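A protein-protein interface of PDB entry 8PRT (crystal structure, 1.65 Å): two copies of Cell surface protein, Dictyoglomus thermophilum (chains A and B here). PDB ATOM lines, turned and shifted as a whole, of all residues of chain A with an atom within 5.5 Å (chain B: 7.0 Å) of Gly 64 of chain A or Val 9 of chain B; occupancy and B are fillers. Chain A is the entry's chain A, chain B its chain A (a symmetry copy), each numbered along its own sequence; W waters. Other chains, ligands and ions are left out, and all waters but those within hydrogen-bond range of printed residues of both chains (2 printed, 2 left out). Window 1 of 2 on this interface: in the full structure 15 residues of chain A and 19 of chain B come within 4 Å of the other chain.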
ATOM      1  N   SER A  48     -12.051  15.072  19.311  1.00  0.00           N
ATOM      2  CA  SER A  48     -11.612  15.376  20.677  1.00  0.00           C
ATOM      3  C   SER A  48     -10.113  15.609  20.765  1.00  0.00           C
ATOM      4  O   SER A  48      -9.315  14.859  20.210  1.00  0.00           O
ATOM      5  CB  SER A  48     -11.986  14.238  21.620  1.00  0.00           C
ATOM      6  OG  SER A  48     -13.399  14.147  21.703  1.00  0.00           O
ATOM      7  N   VAL A  49      -9.730  16.621  21.543  1.00  0.00           N
ATOM      8  CA  VAL A  49      -8.312  16.883  21.779  1.00  0.00           C
ATOM      9  C   VAL A  49      -8.004  16.272  23.138  1.00  0.00           C
ATOM     10  O   VAL A  49      -8.024  16.951  24.176  1.00  0.00           O
ATOM     11  CB  VAL A  49      -7.972  18.380  21.701  1.00  0.00           C
ATOM     12  CG1 VAL A  49      -6.470  18.598  21.879  1.00  0.00           C
ATOM     13  CG2 VAL A  49      -8.390  18.920  20.357  1.00  0.00           C
ATOM     14  N   HIS A  50      -7.774  14.951  23.162  1.00  0.00           N
ATOM     15  CA  HIS A  50      -7.410  14.280  24.406  1.00  0.00           C
ATOM     16  C   HIS A  50      -5.931  14.475  24.704  1.00  0.00           C
ATOM     17  O   HIS A  50      -5.516  14.483  25.870  1.00  0.00           O
ATOM     18  CB  HIS A  50      -7.661  12.767  24.345  1.00  0.00           C
ATOM     19  CG  HIS A  50      -9.100  12.350  24.474  1.00  0.00           C
ATOM     20  ND1 HIS A  50      -9.943  12.234  23.392  1.00  0.00           N
ATOM     21  CD2 HIS A  50      -9.827  11.976  25.557  1.00  0.00           C
ATOM     22  CE1 HIS A  50     -11.129  11.816  23.801  1.00  0.00           C
ATOM     23  NE2 HIS A  50     -11.087  11.659  25.110  1.00  0.00           N
ATOM     24  N   SER A  51      -5.134  14.579  23.650  1.00  0.00           N
ATOM     25  CA  SER A  51      -3.706  14.794  23.779  1.00  0.00           C
ATOM     26  C   SER A  51      -3.427  16.086  24.522  1.00  0.00           C
ATOM     27  O   SER A  51      -4.209  17.033  24.477  1.00  0.00           O
ATOM     28  CB  SER A  51      -3.140  14.822  22.363  1.00  0.00           C
ATOM     29  OG  SER A  51      -1.768  15.118  22.283  1.00  0.00           O
ATOM     30  N   TYR A  62       2.053  22.224  19.989  1.00  0.00           N
ATOM     31  CA  TYR A  62       1.797  20.958  19.311  1.00  0.00           C
ATOM     32  C   TYR A  62       0.816  20.132  20.126  1.00  0.00           C
ATOM     33  O   TYR A  62       0.958  20.024  21.351  1.00  0.00           O
ATOM     34  CB  TYR A  62       3.081  20.145  19.140  1.00  0.00           C
ATOM     35  CG  TYR A  62       4.204  20.895  18.467  1.00  0.00           C
ATOM     36  CD1 TYR A  62       4.318  20.929  17.081  1.00  0.00           C
ATOM     37  CD2 TYR A  62       5.164  21.548  19.224  1.00  0.00           C
ATOM     38  CE1 TYR A  62       5.371  21.629  16.465  1.00  0.00           C
ATOM     39  CE2 TYR A  62       6.192  22.227  18.625  1.00  0.00           C
ATOM     40  CZ  TYR A  62       6.291  22.260  17.255  1.00  0.00           C
ATOM     41  OH  TYR A  62       7.332  22.932  16.659  1.00  0.00           O
ATOM     42  N   VAL A  63      -0.152  19.523  19.443  1.00  0.00           N
ATOM     43  CA  VAL A  63      -1.128  18.685  20.141  1.00  0.00           C
ATOM     44  C   VAL A  63      -1.740  17.709  19.140  1.00  0.00           C
ATOM     45  O   VAL A  63      -1.970  18.044  17.983  1.00  0.00           O
ATOM     46  CB  VAL A  63      -2.204  19.555  20.831  1.00  0.00           C
ATOM     47  CG1 VAL A  63      -3.208  20.085  19.808  1.00  0.00           C
ATOM     48  CG2 VAL A  63      -2.894  18.780  21.945  1.00  0.00           C
ATOM     49  N   GLY A  64      -2.023  16.505  19.619  1.00  0.00           N
ATOM     50  CA  GLY A  64      -2.747  15.550  18.816  1.00  0.00           C
ATOM     51  C   GLY A  64      -4.250  15.702  18.932  1.00  0.00           C
ATOM     52  O   GLY A  64      -4.775  16.336  19.841  1.00  0.00           O
ATOM     53  N   SER A  65      -4.955  15.096  17.979  1.00  0.00           N
ATOM     54  CA  SER A  65      -6.409  15.096  17.987  1.00  0.00           C
ATOM     55  C   SER A  65      -6.906  13.697  17.641  1.00  0.00           C
ATOM     56  O   SER A  65      -6.221  12.935  16.971  1.00  0.00           O
ATOM     57  CB  SER A  65      -6.964  16.118  16.985  1.00  0.00           C
ATOM     58  OG  SER A  65      -8.372  16.021  16.871  1.00  0.00           O
ATOM     59  N   ASN A  66      -8.099  13.366  18.119  1.00  0.00           N
ATOM     60  CA  ASN A  66      -8.711  12.109  17.696  1.00  0.00           C
ATOM     61  C   ASN A  66      -9.120  12.109  16.226  1.00  0.00           C
ATOM     62  O   ASN A  66      -9.538  11.056  15.714  1.00  0.00           O
ATOM     63  CB  ASN A  66      -9.904  11.809  18.595  1.00  0.00           C
ATOM     64  CG  ASN A  66      -9.499  11.347  19.983  1.00  0.00           C
ATOM     65  OD1 ASN A  66      -8.324  11.386  20.356  1.00  0.00           O
ATOM     66  ND2 ASN A  66     -10.487  10.927  20.767  1.00  0.00           N
ATOM     67  N   HIS A  68      -6.976  12.207  13.996  1.00  0.00           N
ATOM     68  CA  HIS A  68      -5.830  11.445  13.507  1.00  0.00           C
ATOM     69  C   HIS A  68      -4.605  12.326  13.257  1.00  0.00           C
ATOM     70  O   HIS A  68      -3.549  11.818  12.887  1.00  0.00           O
ATOM     71  CB  HIS A  68      -6.090  10.662  12.198  1.00  0.00           C
ATOM     72  CG  HIS A  68      -7.206   9.659  12.267  1.00  0.00           C
ATOM     73  ND1 HIS A  68      -7.491   8.805  11.221  1.00  0.00           N
ATOM     74  CD2 HIS A  68      -8.108   9.375  13.238  1.00  0.00           C
ATOM     75  CE1 HIS A  68      -8.526   8.047  11.541  1.00  0.00           C
ATOM     76  NE2 HIS A  68      -8.916   8.366  12.758  1.00  0.00           N
ATOM     77  N   TYR A  69      -4.741  13.644  13.447  1.00  0.00           N
ATOM     78  CA  TYR A  69      -3.644  14.555  13.121  1.00  0.00           C
ATOM     79  C   TYR A  69      -2.884  15.003  14.357  1.00  0.00           C
ATOM     80  O   TYR A  69      -3.449  15.157  15.437  1.00  0.00           O
ATOM     81  CB  TYR A  69      -4.145  15.812  12.400  1.00  0.00           C
ATOM     82  CG  TYR A  69      -4.645  15.594  10.997  1.00  0.00           C
ATOM     83  CD1 TYR A  69      -5.927  15.099  10.754  1.00  0.00           C
ATOM     84  CD2 TYR A  69      -3.850  15.913   9.908  1.00  0.00           C
ATOM     85  CE1 TYR A  69      -6.371  14.908   9.451  1.00  0.00           C
ATOM     86  CE2 TYR A  69      -4.289  15.742   8.632  1.00  0.00           C
ATOM     87  CZ  TYR A  69      -5.540  15.250   8.394  1.00  0.00           C
ATOM     88  OH  TYR A  69      -5.930  15.097   7.074  1.00  0.00           O
ATOM     89  N   LEU A  70      -1.583  15.246  14.168  1.00  0.00           N
ATOM     90  CA  LEU A  70      -0.806  16.096  15.046  1.00  0.00           C
ATOM     91  C   LEU A  70      -0.858  17.510  14.493  1.00  0.00           C
ATOM     92  O   LEU A  70      -0.531  17.730  13.325  1.00  0.00           O
ATOM     93  CB  LEU A  70       0.645  15.627  15.100  1.00  0.00           C
ATOM     94  CG  LEU A  70       1.599  16.539  15.876  1.00  0.00           C
ATOM     95  CD1 LEU A  70       1.255  16.464  17.340  1.00  0.00           C
ATOM     96  CD2 LEU A  70       3.016  16.107  15.604  1.00  0.00           C
ATOM     97  N   TYR A  71      -1.248  18.462  15.338  1.00  0.00           N
ATOM     98  CA  TYR A  71      -1.351  19.858  14.960  1.00  0.00           C
ATOM     99  C   TYR A  71      -0.172  20.633  15.498  1.00  0.00           C
ATOM    100  O   TYR A  71       0.285  20.368  16.611  1.00  0.00           O
ATOM    101  CB  TYR A  71      -2.621  20.455  15.519  1.00  0.00           C
ATOM    102  CG  TYR A  71      -3.837  20.032  14.756  1.00  0.00           C
ATOM    103  CD1 TYR A  71      -4.486  18.832  15.042  1.00  0.00           C
ATOM    104  CD2 TYR A  71      -4.336  20.820  13.742  1.00  0.00           C
ATOM    105  CE1 TYR A  71      -5.611  18.448  14.344  1.00  0.00           C
ATOM    106  CE2 TYR A  71      -5.470  20.440  13.036  1.00  0.00           C
ATOM    107  CZ  TYR A  71      -6.089  19.245  13.342  1.00  0.00           C
ATOM    108  OH  TYR A  71      -7.213  18.873  12.632  1.00  0.00           O
ATOM    109  N   THR B   5      -1.723  11.080  10.940  1.00  0.00           N
ATOM    110  CA  THR B   5      -1.422   9.671  11.289  1.00  0.00           C
ATOM    111  C   THR B   5      -2.577   8.766  10.855  1.00  0.00           C
ATOM    112  O   THR B   5      -3.546   9.272  10.300  1.00  0.00           O
ATOM    113  CB  THR B   5      -1.166   9.424  12.789  1.00  0.00           C
ATOM    114  OG1 THR B   5      -2.381   9.510  13.525  1.00  0.00           O
ATOM    115  CG2 THR B   5      -0.142  10.372  13.371  1.00  0.00           C
ATOM    116  N   GLY B   6      -2.483   7.471  11.123  1.00  0.00           N
ATOM    117  CA  GLY B   6      -3.529   6.532  10.762  1.00  0.00           C
ATOM    118  C   GLY B   6      -4.639   6.334  11.780  1.00  0.00           C
ATOM    119  O   GLY B   6      -5.549   5.516  11.556  1.00  0.00           O
ATOM    120  N   GLY B   7      -4.593   7.035  12.901  1.00  0.00           N
ATOM    121  CA  GLY B   7      -5.577   6.846  13.954  1.00  0.00           C
ATOM    122  C   GLY B   7      -5.455   7.960  14.966  1.00  0.00           C
ATOM    123  O   GLY B   7      -4.624   8.858  14.824  1.00  0.00           O
ATOM    124  N   SER B   8      -6.291   7.885  16.006  1.00  0.00           N
ATOM    125  CA  SER B   8      -6.324   8.949  17.010  1.00  0.00           C
ATOM    126  C   SER B   8      -4.952   9.195  17.610  1.00  0.00           C
ATOM    127  O   SER B   8      -4.240   8.268  17.985  1.00  0.00           O
ATOM    128  CB  SER B   8      -7.297   8.604  18.135  1.00  0.00           C
ATOM    129  OG  SER B   8      -8.605   8.595  17.634  1.00  0.00           O
ATOM    130  N   VAL B   9      -4.605  10.469  17.726  1.00  0.00           N
ATOM    131  CA  VAL B   9      -3.360  10.856  18.397  1.00  0.00           C
ATOM    132  C   VAL B   9      -3.760  11.184  19.833  1.00  0.00           C
ATOM    133  O   VAL B   9      -3.994  12.322  20.225  1.00  0.00           O
ATOM    134  CB  VAL B   9      -2.668  12.011  17.687  1.00  0.00           C
ATOM    135  CG1 VAL B   9      -1.352  12.333  18.388  1.00  0.00           C
ATOM    136  CG2 VAL B   9      -2.407  11.639  16.240  1.00  0.00           C
ATOM    137  N   HIS B  10      -3.812  10.133  20.638  1.00  0.00           N
ATOM    138  CA  HIS B  10      -4.111  10.234  22.043  1.00  0.00           C
ATOM    139  C   HIS B  10      -2.890  10.651  22.839  1.00  0.00           C
ATOM    140  O   HIS B  10      -2.995  11.364  23.851  1.00  0.00           O
ATOM    141  CB  HIS B  10      -4.571   8.876  22.494  1.00  0.00           C
ATOM    142  CG  HIS B  10      -5.339   8.921  23.739  1.00  0.00           C
ATOM    143  ND1 HIS B  10      -6.677   8.616  23.791  1.00  0.00           N
ATOM    144  CD2 HIS B  10      -4.987   9.340  24.971  1.00  0.00           C
ATOM    145  CE1 HIS B  10      -7.098   8.758  25.030  1.00  0.00           C
ATOM    146  NE2 HIS B  10      -6.093   9.196  25.765  1.00  0.00           N
ATOM    147  N   SER B  11      -1.744  10.165  22.399  1.00  0.00           N
ATOM    148  CA  SER B  11      -0.460  10.448  23.004  1.00  0.00           C
ATOM    149  C   SER B  11      -0.179  11.943  22.978  1.00  0.00           C
ATOM    150  O   SER B  11      -0.645  12.675  22.095  1.00  0.00           O
ATOM    151  CB  SER B  11       0.590   9.669  22.202  1.00  0.00           C
ATOM    152  OG  SER B  11       1.908   9.831  22.651  1.00  0.00           O
ATOM    153  N   SER B  12       0.595  12.387  23.954  1.00  0.00           N
ATOM    154  CA  SER B  12       0.988  13.791  24.083  1.00  0.00           C
ATOM    155  C   SER B  12       2.401  13.998  23.555  1.00  0.00           C
ATOM    156  O   SER B  12       3.305  13.233  23.919  1.00  0.00           O
ATOM    157  CB  SER B  12       0.918  14.214  25.547  1.00  0.00           C
ATOM    158  OG  SER B  12      -0.410  14.077  26.039  1.00  0.00           O
ATOM    159  N   PRO B  13       2.635  15.000  22.720  1.00  0.00           N
ATOM    160  CA  PRO B  13       3.950  15.122  22.082  1.00  0.00           C
ATOM    161  C   PRO B  13       5.057  15.487  23.064  1.00  0.00           C
ATOM    162  O   PRO B  13       4.856  16.212  24.044  1.00  0.00           O
ATOM    163  CB  PRO B  13       3.740  16.229  21.043  1.00  0.00           C
ATOM    164  CG  PRO B  13       2.484  16.949  21.463  1.00  0.00           C
ATOM    165  CD  PRO B  13       1.652  15.962  22.178  1.00  0.00           C
ATOM    166  N   VAL B  23       5.486  11.671  18.970  1.00  0.00           N
ATOM    167  CA  VAL B  23       4.145  11.414  19.487  1.00  0.00           C
ATOM    168  C   VAL B  23       3.699  10.044  19.005  1.00  0.00           C
ATOM    169  O   VAL B  23       4.069   9.602  17.923  1.00  0.00           O
ATOM    170  CB  VAL B  23       3.151  12.526  19.071  1.00  0.00           C
ATOM    171  CG1 VAL B  23       2.761  12.408  17.597  1.00  0.00           C
ATOM    172  CG2 VAL B  23       1.917  12.501  19.982  1.00  0.00           C
ATOM    173  N   GLY B  24       2.926   9.369  19.832  1.00  0.00           N
ATOM    174  CA  GLY B  24       2.338   8.107  19.443  1.00  0.00           C
ATOM    175  C   GLY B  24       0.986   8.287  18.821  1.00  0.00           C
ATOM    176  O   GLY B  24       0.384   9.366  18.881  1.00  0.00           O
ATOM    177  N   SER B  25       0.520   7.204  18.194  1.00  0.00           N
ATOM    178  CA  SER B  25      -0.774   7.180  17.537  1.00  0.00           C
ATOM    179  C   SER B  25      -1.436   5.846  17.813  1.00  0.00           C
ATOM    180  O   SER B  25      -0.768   4.839  18.022  1.00  0.00           O
ATOM    181  CB  SER B  25      -0.638   7.384  16.017  1.00  0.00           C
ATOM    182  OG  SER B  25      -1.879   7.207  15.348  1.00  0.00           O
ATOM    183  N   ASN B  26      -2.766   5.855  17.804  1.00  0.00           N
ATOM    184  CA  ASN B  26      -3.485   4.597  17.928  1.00  0.00           C
ATOM    185  C   ASN B  26      -3.314   3.701  16.707  1.00  0.00           C
ATOM    186  O   ASN B  26      -3.802   2.553  16.728  1.00  0.00           O
ATOM    187  CB  ASN B  26      -4.947   4.903  18.181  1.00  0.00           C
ATOM    188  CG  ASN B  26      -5.217   5.378  19.609  1.00  0.00           C
ATOM    189  OD1 ASN B  26      -4.297   5.629  20.389  1.00  0.00           O
ATOM    190  ND2 ASN B  26      -6.488   5.522  19.937  1.00  0.00           N
ATOM    191  N   ASP B  27      -2.658   4.186  15.648  1.00  0.00           N
ATOM    192  CA  ASP B  27      -2.300   3.361  14.502  1.00  0.00           C
ATOM    193  C   ASP B  27      -1.098   2.465  14.772  1.00  0.00           C
ATOM    194  O   ASP B  27      -0.699   1.720  13.871  1.00  0.00           O
ATOM    195  CB  ASP B  27      -2.055   4.236  13.258  1.00  0.00           C
ATOM    196  CG  ASP B  27      -0.751   5.033  13.295  1.00  0.00           C
ATOM    197  OD1 ASP B  27       0.023   4.934  14.264  1.00  0.00           O
ATOM    198  OD2 ASP B  27      -0.515   5.763  12.300  1.00  0.00           O
ATOM    199  N   TYR B  31       5.801   8.386  16.112  1.00  0.00           N
ATOM    200  CA  TYR B  31       6.171   9.290  15.040  1.00  0.00           C
ATOM    201  C   TYR B  31       7.231  10.262  15.520  1.00  0.00           C
ATOM    202  O   TYR B  31       7.153  10.752  16.642  1.00  0.00           O
ATOM    203  CB  TYR B  31       4.967  10.096  14.569  1.00  0.00           C
ATOM    204  CG  TYR B  31       4.022   9.301  13.715  1.00  0.00           C
ATOM    205  CD1 TYR B  31       3.027   8.539  14.284  1.00  0.00           C
ATOM    206  CD2 TYR B  31       4.150   9.288  12.346  1.00  0.00           C
ATOM    207  CE1 TYR B  31       2.175   7.790  13.503  1.00  0.00           C
ATOM    208  CE2 TYR B  31       3.302   8.536  11.556  1.00  0.00           C
ATOM    209  CZ  TYR B  31       2.310   7.786  12.147  1.00  0.00           C
ATOM    210  OH  TYR B  31       1.423   7.017  11.381  1.00  0.00           O
ATOM    211  N   VAL B  49      -0.264   3.398  20.644  1.00  0.00           N
ATOM    212  CA  VAL B  49       0.722   4.101  21.462  1.00  0.00           C
ATOM    213  C   VAL B  49      -0.043   5.221  22.152  1.00  0.00           C
ATOM    214  O   VAL B  49      -0.075   6.370  21.686  1.00  0.00           O
ATOM    215  CB  VAL B  49       1.915   4.607  20.636  1.00  0.00           C
ATOM    216  CG1 VAL B  49       2.953   5.267  21.543  1.00  0.00           C
ATOM    217  CG2 VAL B  49       2.557   3.447  19.919  1.00  0.00           C
HETATM  218  O   HOH W   1      -3.440  13.726  27.437  1.00  0.00           O
HETATM  219  O   HOH W   2      -5.895   8.870   8.935  1.00  0.00           O
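Ser 51 of chain A touches Val 9 of chain B (CB to O, 3.4 Å).
Ser 51 of chain A touches Ser 12 of chain B.
Pro 13 of chain B touches Tyr 62 of chain A.
CG1 of Val 9 of chain B touches CA of Gly 64 of chain A (3.5 Å).
Ser 65 of chain A touches Ser 8 of chain B (O to CA, 3.99 Å).
His 68 of chain A touches Gly 6 of chain B (ND1 to C, 3.8 Å).
His 68 of chain A touches Gly 7 of chain B (CA to O, 3.1 Å).
His 68 of chain A touches Ser 8 of chain B (CD2 to N, 3.6 Å).
His 68 of chain A touches Val 9 of chain B (O to CG2, 3.5 Å).
Val 9 of chain B touches Tyr 69 of chain A.
Ser 48 of chain A touches none of the printed residues of chain B.
Gly 64 of chain A touches just one residue of chain B: Val 9 (3.5 Å).
Of the printed residues of chain A, Thr 5 of chain B touches His 68 (2.7 Å).
Of the printed residues of chain A, Ser 11 of chain B touches Ser 51 (2.7 Å).
Of the printed residues of chain A, Pro 13 of chain B touches Ser 51 (3.5 Å) and Tyr 62 (3.4 Å).
Tyr 31 of chain B touches none of the printed residues of chain A.
The side-chain hydroxyl (OG) of Ser 51 of chain A lies within hydrogen-bond range of the backbone carbonyl oxygen (O) of Ser 11 of chain B, 2.7 Å away.
The backbone carbonyl oxygen of Ser 65 of chain A is in hydrogen-bond range of the backbone NH of Val 9 of chain B, at 3.0 Å.
O of Asn 66 of chain A sits at hydrogen-bond distance from OG of Ser 8 of chain B (3.3 Å).
O of His 68 of chain A is in hydrogen-bond range of OG1 of Thr 5 of chain B (2.7 Å).
Water W1 bridges O of His 50 of chain A (2.7 Å) and OG of Ser 12 of chain B (3.4 Å).
Water W2 lies within hydrogen-bond range of O of Thr 5 of chain B (2.7 Å) and ND1 of His 68 of chain A (2.8 Å).
Position printed for both chains: 49.
The backbone NH (N) of Asn 66 of chain A is in hydrogen-bond range of the backbone carbonyl oxygen (O) of Ser 48 of chain A (2.8 Å).
The backbone carbonyl oxygen (O) of Gly 7 of chain B is in hydrogen-bond range of the side-chain hydroxyl (OG1) of Thr 5 of chain B, 2.7 Å away.
OG1 of Thr 5 of chain B sits at hydrogen-bond distance from OG of Ser 25 of chain B.
The backbone NH of Gly 6 of chain B sits at hydrogen-bond distance from the side-chain carboxylate of Asp 27 of chain B (2.9 Å).
O of Gly 7 of chain B sits at hydrogen-bond distance from OG of Ser 25 of chain B (3.2 Å).
The backbone carbonyl oxygen (O) of Ser 8 of chain B lies within hydrogen-bond range of the backbone NH (N) of Asn 26 of chain B (2.8 Å).
Printed residues of chain B that touch a printed residue of chain A: Thr 5, Gly 6, Gly 7, Ser 8, Val 9, His 10, Ser 11, Ser 12 and Pro 13.
Hydrophobic or aromatic side chains of chain B that line the printed part of chain A: Val 9 and Pro 13.
Hydrophobic or aromatic side chains of chain A within 4 Å of the printed part of chain B: Tyr 62 and His 68.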
